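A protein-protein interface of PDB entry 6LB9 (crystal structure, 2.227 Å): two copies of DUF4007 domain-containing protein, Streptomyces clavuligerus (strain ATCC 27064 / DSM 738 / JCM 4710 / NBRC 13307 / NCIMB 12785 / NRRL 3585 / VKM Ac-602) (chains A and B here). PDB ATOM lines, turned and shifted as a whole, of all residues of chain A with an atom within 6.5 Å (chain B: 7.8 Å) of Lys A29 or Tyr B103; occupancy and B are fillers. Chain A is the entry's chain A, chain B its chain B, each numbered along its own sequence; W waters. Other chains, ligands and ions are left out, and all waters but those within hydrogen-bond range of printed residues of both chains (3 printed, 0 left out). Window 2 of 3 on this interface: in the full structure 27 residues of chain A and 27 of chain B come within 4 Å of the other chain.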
ATOM      1  N   PHE A  24      10.586 -17.323   9.174  1.00  0.00           N
ATOM      2  CA  PHE A  24       9.357 -17.089   9.910  1.00  0.00           C
ATOM      3  C   PHE A  24       9.391 -15.744  10.632  1.00  0.00           C
ATOM      4  O   PHE A  24       8.384 -15.024  10.652  1.00  0.00           O
ATOM      5  CB  PHE A  24       9.082 -18.195  10.927  1.00  0.00           C
ATOM      6  CG  PHE A  24       8.081 -17.766  11.951  1.00  0.00           C
ATOM      7  CD1 PHE A  24       6.741 -17.672  11.603  1.00  0.00           C
ATOM      8  CD2 PHE A  24       8.487 -17.330  13.215  1.00  0.00           C
ATOM      9  CE1 PHE A  24       5.807 -17.232  12.528  1.00  0.00           C
ATOM     10  CE2 PHE A  24       7.558 -16.885  14.139  1.00  0.00           C
ATOM     11  CZ  PHE A  24       6.223 -16.813  13.794  1.00  0.00           C
ATOM     12  N   GLY A  25      10.526 -15.401  11.264  1.00  0.00           N
ATOM     13  CA  GLY A  25      10.602 -14.125  11.960  1.00  0.00           C
ATOM     14  C   GLY A  25      10.344 -12.949  11.034  1.00  0.00           C
ATOM     15  O   GLY A  25       9.749 -11.949  11.434  1.00  0.00           O
ATOM     16  N   TRP A  26      10.748 -13.075   9.774  1.00  0.00           N
ATOM     17  CA  TRP A  26      10.546 -12.006   8.812  1.00  0.00           C
ATOM     18  C   TRP A  26       9.072 -11.824   8.500  1.00  0.00           C
ATOM     19  O   TRP A  26       8.570 -10.695   8.470  1.00  0.00           O
ATOM     20  CB  TRP A  26      11.338 -12.307   7.544  1.00  0.00           C
ATOM     21  CG  TRP A  26      12.793 -12.015   7.674  1.00  0.00           C
ATOM     22  CD1 TRP A  26      13.445 -11.611   8.796  1.00  0.00           C
ATOM     23  CD2 TRP A  26      13.784 -12.097   6.638  1.00  0.00           C
ATOM     24  NE1 TRP A  26      14.779 -11.436   8.532  1.00  0.00           N
ATOM     25  CE2 TRP A  26      15.016 -11.723   7.213  1.00  0.00           C
ATOM     26  CE3 TRP A  26      13.746 -12.436   5.282  1.00  0.00           C
ATOM     27  CZ2 TRP A  26      16.211 -11.690   6.480  1.00  0.00           C
ATOM     28  CZ3 TRP A  26      14.931 -12.399   4.549  1.00  0.00           C
ATOM     29  CH2 TRP A  26      16.144 -12.032   5.153  1.00  0.00           C
ATOM     30  N   LEU A  27       8.364 -12.929   8.248  1.00  0.00           N
ATOM     31  CA  LEU A  27       6.927 -12.856   8.020  1.00  0.00           C
ATOM     32  C   LEU A  27       6.214 -12.255   9.224  1.00  0.00           C
ATOM     33  O   LEU A  27       5.379 -11.360   9.074  1.00  0.00           O
ATOM     34  CB  LEU A  27       6.375 -14.258   7.695  1.00  0.00           C
ATOM     35  CG  LEU A  27       6.990 -14.947   6.467  1.00  0.00           C
ATOM     36  CD1 LEU A  27       6.237 -16.212   6.088  1.00  0.00           C
ATOM     37  CD2 LEU A  27       7.086 -13.975   5.273  1.00  0.00           C
ATOM     38  N   HIS A  28       6.563 -12.714  10.429  1.00  0.00           N
ATOM     39  CA  HIS A  28       5.841 -12.337  11.642  1.00  0.00           C
ATOM     40  C   HIS A  28       6.086 -10.872  12.003  1.00  0.00           C
ATOM     41  O   HIS A  28       5.139 -10.118  12.258  1.00  0.00           O
ATOM     42  CB  HIS A  28       6.272 -13.263  12.782  1.00  0.00           C
ATOM     43  CG  HIS A  28       5.792 -12.849  14.138  1.00  0.00           C
ATOM     44  ND1 HIS A  28       4.477 -12.958  14.535  1.00  0.00           N
ATOM     45  CD2 HIS A  28       6.467 -12.370  15.212  1.00  0.00           C
ATOM     46  CE1 HIS A  28       4.357 -12.548  15.784  1.00  0.00           C
ATOM     47  NE2 HIS A  28       5.552 -12.190  16.220  1.00  0.00           N
ATOM     48  N   LYS A  29       7.353 -10.449  12.028  1.00  0.00           N
ATOM     49  CA  LYS A  29       7.640  -9.070  12.416  1.00  0.00           C
ATOM     50  C   LYS A  29       7.163  -8.088  11.357  1.00  0.00           C
ATOM     51  O   LYS A  29       6.609  -7.040  11.693  1.00  0.00           O
ATOM     52  CB  LYS A  29       9.131  -8.895  12.710  1.00  0.00           C
ATOM     53  CG  LYS A  29       9.553  -9.677  13.955  1.00  0.00           C
ATOM     54  CD  LYS A  29      10.997  -9.439  14.352  1.00  0.00           C
ATOM     55  CE  LYS A  29      11.988 -10.107  13.389  1.00  0.00           C
ATOM     56  NZ  LYS A  29      13.389  -9.771  13.799  1.00  0.00           N
ATOM     57  N   ALA A  30       7.321  -8.425  10.073  1.00  0.00           N
ATOM     58  CA  ALA A  30       6.830  -7.519   9.035  1.00  0.00           C
ATOM     59  C   ALA A  30       5.326  -7.291   9.179  1.00  0.00           C
ATOM     60  O   ALA A  30       4.851  -6.152   9.052  1.00  0.00           O
ATOM     61  CB  ALA A  30       7.184  -8.049   7.639  1.00  0.00           C
ATOM     62  N   TYR A  31       4.562  -8.357   9.468  1.00  0.00           N
ATOM     63  CA  TYR A  31       3.133  -8.197   9.744  1.00  0.00           C
ATOM     64  C   TYR A  31       2.880  -7.311  10.966  1.00  0.00           C
ATOM     65  O   TYR A  31       1.987  -6.458  10.949  1.00  0.00           O
ATOM     66  CB  TYR A  31       2.444  -9.552   9.952  1.00  0.00           C
ATOM     67  CG  TYR A  31       1.002  -9.342  10.359  1.00  0.00           C
ATOM     68  CD1 TYR A  31       0.046  -8.964   9.416  1.00  0.00           C
ATOM     69  CD2 TYR A  31       0.603  -9.455  11.692  1.00  0.00           C
ATOM     70  CE1 TYR A  31      -1.269  -8.733   9.780  1.00  0.00           C
ATOM     71  CE2 TYR A  31      -0.709  -9.244  12.061  1.00  0.00           C
ATOM     72  CZ  TYR A  31      -1.642  -8.873  11.101  1.00  0.00           C
ATOM     73  OH  TYR A  31      -2.955  -8.635  11.459  1.00  0.00           O
ATOM     74  N   MET A  32       3.621  -7.530  12.053  1.00  0.00           N
ATOM     75  CA  MET A  32       3.365  -6.774  13.279  1.00  0.00           C
ATOM     76  C   MET A  32       3.540  -5.273  13.051  1.00  0.00           C
ATOM     77  O   MET A  32       2.785  -4.464  13.597  1.00  0.00           O
ATOM     78  CB  MET A  32       4.302  -7.251  14.394  1.00  0.00           C
ATOM     79  CG  MET A  32       4.012  -8.638  14.963  1.00  0.00           C
ATOM     80  SD  MET A  32       2.386  -8.698  15.737  1.00  0.00           S
ATOM     81  CE  MET A  32       2.703  -7.766  17.246  1.00  0.00           C
ATOM     82  N   GLN A  33       4.526  -4.894  12.238  1.00  0.00           N
ATOM     83  CA  GLN A  33       4.920  -3.522  11.956  1.00  0.00           C
ATOM     84  C   GLN A  33       4.100  -2.873  10.837  1.00  0.00           C
ATOM     85  O   GLN A  33       3.696  -1.709  10.956  1.00  0.00           O
ATOM     86  CB  GLN A  33       6.400  -3.473  11.564  1.00  0.00           C
ATOM     87  CG  GLN A  33       7.391  -3.936  12.622  1.00  0.00           C
ATOM     88  CD  GLN A  33       7.531  -2.928  13.733  1.00  0.00           C
ATOM     89  OE1 GLN A  33       7.891  -1.768  13.502  1.00  0.00           O
ATOM     90  NE2 GLN A  33       7.269  -3.370  14.960  1.00  0.00           N
ATOM     91  N   VAL A  34       3.904  -3.574   9.720  1.00  0.00           N
ATOM     92  CA  VAL A  34       3.182  -2.980   8.596  1.00  0.00           C
ATOM     93  C   VAL A  34       1.721  -2.711   8.954  1.00  0.00           C
ATOM     94  O   VAL A  34       1.073  -1.857   8.335  1.00  0.00           O
ATOM     95  CB  VAL A  34       3.297  -3.892   7.357  1.00  0.00           C
ATOM     96  CG1 VAL A  34       2.263  -5.026   7.428  1.00  0.00           C
ATOM     97  CG2 VAL A  34       3.101  -3.089   6.103  1.00  0.00           C
ATOM     98  N   GLN A  49      13.813  -1.170  14.122  1.00  0.00           N
ATOM     99  CA  GLN A  49      12.418  -1.446  14.447  1.00  0.00           C
ATOM    100  C   GLN A  49      11.939  -2.788  13.888  1.00  0.00           C
ATOM    101  O   GLN A  49      11.045  -3.395  14.470  1.00  0.00           O
ATOM    102  CB  GLN A  49      11.542  -0.293  13.981  1.00  0.00           C
ATOM    103  CG  GLN A  49      12.070   1.050  14.487  1.00  0.00           C
ATOM    104  CD  GLN A  49      11.468   2.253  13.780  1.00  0.00           C
ATOM    105  OE1 GLN A  49      11.487   3.367  14.320  1.00  0.00           O
ATOM    106  NE2 GLN A  49      10.939   2.047  12.571  1.00  0.00           N
ATOM    107  N   LEU A  50      12.529  -3.282  12.798  1.00  0.00           N
ATOM    108  CA  LEU A  50      12.200  -4.597  12.264  1.00  0.00           C
ATOM    109  C   LEU A  50      13.111  -5.700  12.802  1.00  0.00           C
ATOM    110  O   LEU A  50      12.869  -6.878  12.512  1.00  0.00           O
ATOM    111  CB  LEU A  50      12.266  -4.580  10.724  1.00  0.00           C
ATOM    112  CG  LEU A  50      11.221  -3.802   9.900  1.00  0.00           C
ATOM    113  CD1 LEU A  50      11.693  -3.628   8.454  1.00  0.00           C
ATOM    114  CD2 LEU A  50       9.840  -4.474   9.916  1.00  0.00           C
ATOM    115  N   GLY A  51      14.151  -5.346  13.556  1.00  0.00           N
ATOM    116  CA  GLY A  51      15.092  -6.302  14.127  1.00  0.00           C
ATOM    117  C   GLY A  51      15.933  -7.075  13.130  1.00  0.00           C
ATOM    118  O   GLY A  51      16.116  -8.290  13.290  1.00  0.00           O
ATOM    119  N   VAL A  52      16.456  -6.409  12.098  1.00  0.00           N
ATOM    120  CA  VAL A  52      17.231  -7.074  11.054  1.00  0.00           C
ATOM    121  C   VAL A  52      18.365  -6.161  10.610  1.00  0.00           C
ATOM    122  O   VAL A  52      18.357  -4.952  10.852  1.00  0.00           O
ATOM    123  CB  VAL A  52      16.360  -7.449   9.833  1.00  0.00           C
ATOM    124  CG1 VAL A  52      15.256  -8.424  10.225  1.00  0.00           C
ATOM    125  CG2 VAL A  52      15.749  -6.209   9.218  1.00  0.00           C
ATOM    126  N   MET A  60      13.121  -8.842   3.286  1.00  0.00           N
ATOM    127  CA  MET A  60      11.966  -8.988   4.157  1.00  0.00           C
ATOM    128  C   MET A  60      10.732  -8.332   3.550  1.00  0.00           C
ATOM    129  O   MET A  60       9.641  -8.915   3.549  1.00  0.00           O
ATOM    130  CB  MET A  60      12.312  -8.376   5.509  1.00  0.00           C
ATOM    131  CG  MET A  60      11.258  -8.442   6.573  1.00  0.00           C
ATOM    132  SD  MET A  60      11.899  -7.545   8.009  1.00  0.00           S
ATOM    133  CE  MET A  60      10.823  -8.138   9.290  1.00  0.00           C
ATOM    134  N   TYR A 103       2.244 -18.722  14.424  1.00  0.00           N
ATOM    135  CA  TYR A 103       3.607 -19.213  14.584  1.00  0.00           C
ATOM    136  C   TYR A 103       3.932 -20.354  13.620  1.00  0.00           C
ATOM    137  O   TYR A 103       4.941 -21.042  13.795  1.00  0.00           O
ATOM    138  CB  TYR A 103       3.832 -19.587  16.057  1.00  0.00           C
ATOM    139  CG  TYR A 103       3.746 -18.331  16.909  1.00  0.00           C
ATOM    140  CD1 TYR A 103       4.696 -17.318  16.759  1.00  0.00           C
ATOM    141  CD2 TYR A 103       2.699 -18.110  17.795  1.00  0.00           C
ATOM    142  CE1 TYR A 103       4.630 -16.124  17.494  1.00  0.00           C
ATOM    143  CE2 TYR A 103       2.622 -16.896  18.555  1.00  0.00           C
ATOM    144  CZ  TYR A 103       3.597 -15.920  18.383  1.00  0.00           C
ATOM    145  OH  TYR A 103       3.584 -14.735  19.081  1.00  0.00           O
ATOM    146  N   SER A 199      17.660 -21.310   9.280  1.00  0.00           N
ATOM    147  CA  SER A 199      16.461 -22.142   9.241  1.00  0.00           C
ATOM    148  C   SER A 199      15.553 -21.702   8.097  1.00  0.00           C
ATOM    149  O   SER A 199      15.478 -20.517   7.751  1.00  0.00           O
ATOM    150  CB  SER A 199      15.677 -22.022  10.555  1.00  0.00           C
ATOM    151  OG  SER A 199      16.353 -22.664  11.612  1.00  0.00           O
ATOM    152  N   PHE B  24       8.046 -23.945  18.105  1.00  0.00           N
ATOM    153  CA  PHE B  24       8.619 -22.621  18.334  1.00  0.00           C
ATOM    154  C   PHE B  24       7.648 -21.712  19.084  1.00  0.00           C
ATOM    155  O   PHE B  24       8.031 -21.039  20.046  1.00  0.00           O
ATOM    156  CB  PHE B  24       9.038 -21.934  17.044  1.00  0.00           C
ATOM    157  CG  PHE B  24       9.397 -20.505  17.279  1.00  0.00           C
ATOM    158  CD1 PHE B  24      10.549 -20.193  17.984  1.00  0.00           C
ATOM    159  CD2 PHE B  24       8.538 -19.477  16.909  1.00  0.00           C
ATOM    160  CE1 PHE B  24      10.885 -18.861  18.265  1.00  0.00           C
ATOM    161  CE2 PHE B  24       8.862 -18.131  17.190  1.00  0.00           C
ATOM    162  CZ  PHE B  24      10.033 -17.831  17.864  1.00  0.00           C
ATOM    163  N   HIS B  28       8.449 -19.461  22.473  1.00  0.00           N
ATOM    164  CA  HIS B  28       8.321 -18.006  22.438  1.00  0.00           C
ATOM    165  C   HIS B  28       7.284 -17.523  23.449  1.00  0.00           C
ATOM    166  O   HIS B  28       7.570 -16.663  24.290  1.00  0.00           O
ATOM    167  CB  HIS B  28       7.959 -17.579  21.011  1.00  0.00           C
ATOM    168  CG  HIS B  28       7.755 -16.107  20.835  1.00  0.00           C
ATOM    169  ND1 HIS B  28       8.787 -15.194  20.880  1.00  0.00           N
ATOM    170  CD2 HIS B  28       6.633 -15.391  20.581  1.00  0.00           C
ATOM    171  CE1 HIS B  28       8.312 -13.982  20.669  1.00  0.00           C
ATOM    172  NE2 HIS B  28       7.007 -14.073  20.481  1.00  0.00           N
ATOM    173  N   MET B  32       7.605 -15.218  27.071  1.00  0.00           N
ATOM    174  CA  MET B  32       6.974 -13.912  27.217  1.00  0.00           C
ATOM    175  C   MET B  32       6.057 -13.861  28.439  1.00  0.00           C
ATOM    176  O   MET B  32       6.086 -12.892  29.199  1.00  0.00           O
ATOM    177  CB  MET B  32       6.202 -13.539  25.951  1.00  0.00           C
ATOM    178  CG  MET B  32       7.065 -13.336  24.709  1.00  0.00           C
ATOM    179  SD  MET B  32       8.582 -12.390  25.074  1.00  0.00           S
ATOM    180  CE  MET B  32       7.971 -10.821  25.721  1.00  0.00           C
ATOM    181  N   LEU B  94      18.655 -15.560  25.012  1.00  0.00           N
ATOM    182  CA  LEU B  94      18.373 -16.145  23.703  1.00  0.00           C
ATOM    183  C   LEU B  94      17.069 -15.645  23.087  1.00  0.00           C
ATOM    184  O   LEU B  94      17.045 -15.233  21.919  1.00  0.00           O
ATOM    185  CB  LEU B  94      18.330 -17.677  23.819  1.00  0.00           C
ATOM    186  CG  LEU B  94      17.917 -18.452  22.563  1.00  0.00           C
ATOM    187  CD1 LEU B  94      19.046 -18.364  21.491  1.00  0.00           C
ATOM    188  CD2 LEU B  94      17.550 -19.926  22.908  1.00  0.00           C
ATOM    189  N   LEU B  95      15.977 -15.688  23.855  1.00  0.00           N
ATOM    190  CA  LEU B  95      14.622 -15.617  23.329  1.00  0.00           C
ATOM    191  C   LEU B  95      13.991 -14.253  23.488  1.00  0.00           C
ATOM    192  O   LEU B  95      12.890 -14.036  22.969  1.00  0.00           O
ATOM    193  CB  LEU B  95      13.729 -16.641  24.030  1.00  0.00           C
ATOM    194  CG  LEU B  95      14.203 -18.080  23.819  1.00  0.00           C
ATOM    195  CD1 LEU B  95      13.274 -19.047  24.512  1.00  0.00           C
ATOM    196  CD2 LEU B  95      14.252 -18.359  22.321  1.00  0.00           C
ATOM    197  N   ASP B  96      14.636 -13.351  24.215  1.00  0.00           N
ATOM    198  CA  ASP B  96      14.065 -12.034  24.395  1.00  0.00           C
ATOM    199  C   ASP B  96      14.010 -11.326  23.049  1.00  0.00           C
ATOM    200  O   ASP B  96      14.812 -11.601  22.157  1.00  0.00           O
ATOM    201  CB  ASP B  96      14.893 -11.249  25.408  1.00  0.00           C
ATOM    202  CG  ASP B  96      14.145 -10.038  25.952  1.00  0.00           C
ATOM    203  OD1 ASP B  96      14.239  -8.965  25.312  1.00  0.00           O
ATOM    204  OD2 ASP B  96      13.458 -10.167  26.989  1.00  0.00           O
ATOM    205  N   GLU B  97      13.036 -10.433  22.893  1.00  0.00           N
ATOM    206  CA  GLU B  97      12.951  -9.653  21.659  1.00  0.00           C
ATOM    207  C   GLU B  97      14.269  -8.945  21.370  1.00  0.00           C
ATOM    208  O   GLU B  97      14.620  -8.724  20.209  1.00  0.00           O
ATOM    209  CB  GLU B  97      11.815  -8.625  21.747  1.00  0.00           C
ATOM    210  CG  GLU B  97      10.412  -9.122  21.319  1.00  0.00           C
ATOM    211  CD  GLU B  97      10.393  -9.967  20.033  1.00  0.00           C
ATOM    212  OE1 GLU B  97      10.314 -11.210  20.156  1.00  0.00           O
ATOM    213  OE2 GLU B  97      10.443  -9.398  18.909  1.00  0.00           O
ATOM    214  N   GLY B  99      17.179 -10.360  22.303  1.00  0.00           N
ATOM    215  CA  GLY B  99      18.171 -11.391  22.539  1.00  0.00           C
ATOM    216  C   GLY B  99      18.930 -11.835  21.301  1.00  0.00           C
ATOM    217  O   GLY B  99      18.911 -11.181  20.254  1.00  0.00           O
ATOM    218  N   ALA B 100      19.593 -13.000  21.436  1.00  0.00           N
ATOM    219  CA  ALA B 100      20.484 -13.519  20.395  1.00  0.00           C
ATOM    220  C   ALA B 100      19.721 -13.958  19.154  1.00  0.00           C
ATOM    221  O   ALA B 100      20.175 -13.720  18.028  1.00  0.00           O
ATOM    222  CB  ALA B 100      21.299 -14.699  20.937  1.00  0.00           C
ATOM    223  N   ASP B 101      18.589 -14.654  19.338  1.00  0.00           N
ATOM    224  CA  ASP B 101      17.865 -15.242  18.224  1.00  0.00           C
ATOM    225  C   ASP B 101      16.423 -15.540  18.621  1.00  0.00           C
ATOM    226  O   ASP B 101      16.021 -16.706  18.634  1.00  0.00           O
ATOM    227  CB  ASP B 101      18.563 -16.523  17.748  1.00  0.00           C
ATOM    228  CG  ASP B 101      18.071 -16.984  16.369  1.00  0.00           C
ATOM    229  OD1 ASP B 101      17.266 -16.250  15.749  1.00  0.00           O
ATOM    230  OD2 ASP B 101      18.498 -18.068  15.903  1.00  0.00           O
ATOM    231  N   PRO B 102      15.614 -14.513  18.900  1.00  0.00           N
ATOM    232  CA  PRO B 102      14.260 -14.753  19.443  1.00  0.00           C
ATOM    233  C   PRO B 102      13.361 -15.587  18.543  1.00  0.00           C
ATOM    234  O   PRO B 102      12.445 -16.247  19.044  1.00  0.00           O
ATOM    235  CB  PRO B 102      13.696 -13.334  19.623  1.00  0.00           C
ATOM    236  CG  PRO B 102      14.526 -12.463  18.677  1.00  0.00           C
ATOM    237  CD  PRO B 102      15.881 -13.081  18.624  1.00  0.00           C
ATOM    238  N   TYR B 103      13.593 -15.599  17.236  1.00  0.00           N
ATOM    239  CA  TYR B 103      12.745 -16.353  16.324  1.00  0.00           C
ATOM    240  C   TYR B 103      13.438 -17.578  15.754  1.00  0.00           C
ATOM    241  O   TYR B 103      12.956 -18.145  14.768  1.00  0.00           O
ATOM    242  CB  TYR B 103      12.234 -15.434  15.214  1.00  0.00           C
ATOM    243  CG  TYR B 103      11.310 -14.390  15.811  1.00  0.00           C
ATOM    244  CD1 TYR B 103       9.999 -14.711  16.109  1.00  0.00           C
ATOM    245  CD2 TYR B 103      11.780 -13.128  16.169  1.00  0.00           C
ATOM    246  CE1 TYR B 103       9.151 -13.803  16.690  1.00  0.00           C
ATOM    247  CE2 TYR B 103      10.937 -12.192  16.764  1.00  0.00           C
ATOM    248  CZ  TYR B 103       9.617 -12.545  17.015  1.00  0.00           C
ATOM    249  OH  TYR B 103       8.741 -11.658  17.594  1.00  0.00           O
ATOM    250  N   LEU B 104      14.551 -18.001  16.370  1.00  0.00           N
ATOM    251  CA  LEU B 104      15.297 -19.196  15.961  1.00  0.00           C
ATOM    252  C   LEU B 104      15.572 -19.188  14.456  1.00  0.00           C
ATOM    253  O   LEU B 104      15.334 -20.167  13.744  1.00  0.00           O
ATOM    254  CB  LEU B 104      14.559 -20.474  16.387  1.00  0.00           C
ATOM    255  CG  LEU B 104      14.221 -20.537  17.895  1.00  0.00           C
ATOM    256  CD1 LEU B 104      13.733 -21.946  18.307  1.00  0.00           C
ATOM    257  CD2 LEU B 104      15.380 -20.083  18.769  1.00  0.00           C
ATOM    258  N   GLU B 105      16.093 -18.059  13.971  1.00  0.00           N
ATOM    259  CA  GLU B 105      16.393 -17.906  12.550  1.00  0.00           C
ATOM    260  C   GLU B 105      17.639 -18.666  12.125  1.00  0.00           C
ATOM    261  O   GLU B 105      17.789 -18.991  10.934  1.00  0.00           O
ATOM    262  CB  GLU B 105      16.552 -16.421  12.220  1.00  0.00           C
ATOM    263  CG  GLU B 105      15.307 -15.633  12.575  1.00  0.00           C
ATOM    264  CD  GLU B 105      15.329 -14.175  12.106  1.00  0.00           C
ATOM    265  OE1 GLU B 105      16.420 -13.640  11.786  1.00  0.00           O
ATOM    266  OE2 GLU B 105      14.230 -13.568  12.066  1.00  0.00           O
ATOM    267  N   GLU B 106      18.532 -18.950  13.064  1.00  0.00           N
ATOM    268  CA  GLU B 106      19.808 -19.575  12.768  1.00  0.00           C
ATOM    269  C   GLU B 106      19.802 -21.012  13.260  1.00  0.00           C
ATOM    270  O   GLU B 106      19.359 -21.287  14.380  1.00  0.00           O
ATOM    271  CB  GLU B 106      20.958 -18.790  13.409  1.00  0.00           C
ATOM    272  CG  GLU B 106      21.647 -17.875  12.390  1.00  0.00           C
ATOM    273  CD  GLU B 106      22.698 -16.966  12.987  1.00  0.00           C
ATOM    274  OE1 GLU B 106      23.778 -17.484  13.367  1.00  0.00           O
ATOM    275  OE2 GLU B 106      22.456 -15.734  13.051  1.00  0.00           O
ATOM    276  N   SER B 109      21.179 -22.024  16.621  1.00  0.00           N
ATOM    277  CA  SER B 109      20.362 -21.846  17.824  1.00  0.00           C
ATOM    278  C   SER B 109      19.627 -23.123  18.185  1.00  0.00           C
ATOM    279  O   SER B 109      19.437 -23.415  19.368  1.00  0.00           O
ATOM    280  CB  SER B 109      19.341 -20.720  17.637  1.00  0.00           C
ATOM    281  OG  SER B 109      19.958 -19.472  17.413  1.00  0.00           O
ATOM    282  N   LEU B 110      19.154 -23.863  17.176  1.00  0.00           N
ATOM    283  CA  LEU B 110      18.550 -25.169  17.426  1.00  0.00           C
ATOM    284  C   LEU B 110      19.582 -26.160  17.932  1.00  0.00           C
ATOM    285  O   LEU B 110      19.293 -26.956  18.828  1.00  0.00           O
ATOM    286  CB  LEU B 110      17.872 -25.690  16.156  1.00  0.00           C
ATOM    287  CG  LEU B 110      16.762 -24.739  15.703  1.00  0.00           C
ATOM    288  CD1 LEU B 110      16.323 -25.081  14.315  1.00  0.00           C
ATOM    289  CD2 LEU B 110      15.587 -24.778  16.695  1.00  0.00           C
ATOM    290  N   PRO B 201      11.074 -27.654  14.578  1.00  0.00           N
ATOM    291  CA  PRO B 201      12.296 -27.113  13.970  1.00  0.00           C
ATOM    292  C   PRO B 201      13.526 -27.961  14.193  1.00  0.00           C
ATOM    293  O   PRO B 201      14.518 -27.762  13.489  1.00  0.00           O
ATOM    294  CB  PRO B 201      12.452 -25.737  14.642  1.00  0.00           C
ATOM    295  CG  PRO B 201      11.765 -25.891  15.926  1.00  0.00           C
ATOM    296  CD  PRO B 201      10.578 -26.799  15.665  1.00  0.00           C
HETATM  297  O   HOH W   1      15.583 -18.583   9.417  1.00  0.00           O
HETATM  298  O   HOH W   2      12.483 -17.399  12.102  1.00  0.00           O
HETATM  299  O   HOH W   3      16.521 -11.174  10.905  1.00  0.00           O
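OG of Ser A199 sits at hydrogen-bond distance from O of Leu B104 (3.4 Å).
O of Glu B105 sits at hydrogen-bond distance from N of Ser A199 (2.9 Å).
The side-chain carboxylate of Glu B97 lies within hydrogen-bond range of the side-chain hydroxyl of Tyr B103 (3.0 Å).
The side-chain amino group (NZ) of Lys A29 lies within hydrogen-bond range of the backbone carbonyl oxygen (O) of Leu A50 (3.2 Å).
OD1 of Asp B101 lies within hydrogen-bond range of N of Leu B104 (3.3 Å).
The backbone carbonyl oxygen of Gly A51 sits at hydrogen-bond distance from the side-chain amino group of Lys A29.
The side-chain carboxylate of Asp B101 sits at hydrogen-bond distance from the backbone NH of Glu B105 (2.8 Å).
Lys A29 touches one residue of chain B.
Tyr B103 touches just these residues of chain A: Phe A24, Gly A25, His A28 and Lys A29.
Of the printed residues of chain A, Glu B105 touches Gly A25 (3.7 Å), Trp A26 (3.9 Å) and Ser A199 (2.9 Å).
Of the printed residues of chain A, His B28 touches Tyr A103.
Of the printed residues of chain B, His A28 touches Tyr B103.
Val A52 touches none of the printed residues of chain B.
The nearest residue of chain B that does not touch Lys A29 is Glu B105 (4.3 Å).
Phe A24 touches its own counterpart, Phe B24.
Phe A24 touches Tyr B103, but with the chains exchanged Tyr A103 does not touch Phe B24 (4.3 Å).
His A28 touches Tyr B103, and with the chains exchanged Tyr A103 touches His B28.
4 positions are printed for both chains.
Of the 11 pairs that touch across the chains among the printed residues, 3 have their exchanged pair printed and touching as well.
Among the printed residues, merely in contact across the chains: His A28 with Tyr B103, Tyr A103 with His B28, Phe A24 with Phe B24, Ser A199 with Leu B110, Lys A29 with Tyr B103, Gly A25 with Glu B105, Phe A24 with Tyr B103, Gly A25 with Tyr B103 and Trp A26 with Glu B105.
Of the 18 printed residues of chain A, 7 touch a printed residue of chain B.
Hydrophobic or aromatic side chains of chain A within 4 Å of the printed part of chain B: Phe A24, Trp A26, His A28 and Tyr A103.
Along chain A the printed residues that touch a printed residue of chain B span positions 24 to 199.
Among the printed residues, 11 pairs touch across the chains.
Among the printed residues, no Asp or Glu carboxylate lies within 4 Å of a Lys or Arg side-chain nitrogen of the other chain.
Water W1 lies within hydrogen-bond range of the backbone carbonyl oxygen of Ser A199 (2.6 Å) and the backbone carbonyl oxygen of Glu B105 (2.7 Å).
Water W3 lies within hydrogen-bond range of the side-chain carboxylate (OE1) of Glu B105 (2.6 Å) and the indole nitrogen (NE1) of Trp A26 (3.0 Å).
Water W2 lies within hydrogen-bond range of the backbone carbonyl oxygen (O) of Tyr B103 (2.8 Å), the backbone NH (N) of Gly A25 (2.9 Å) and the backbone NH (N) of Phe A24 (3.5 Å).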
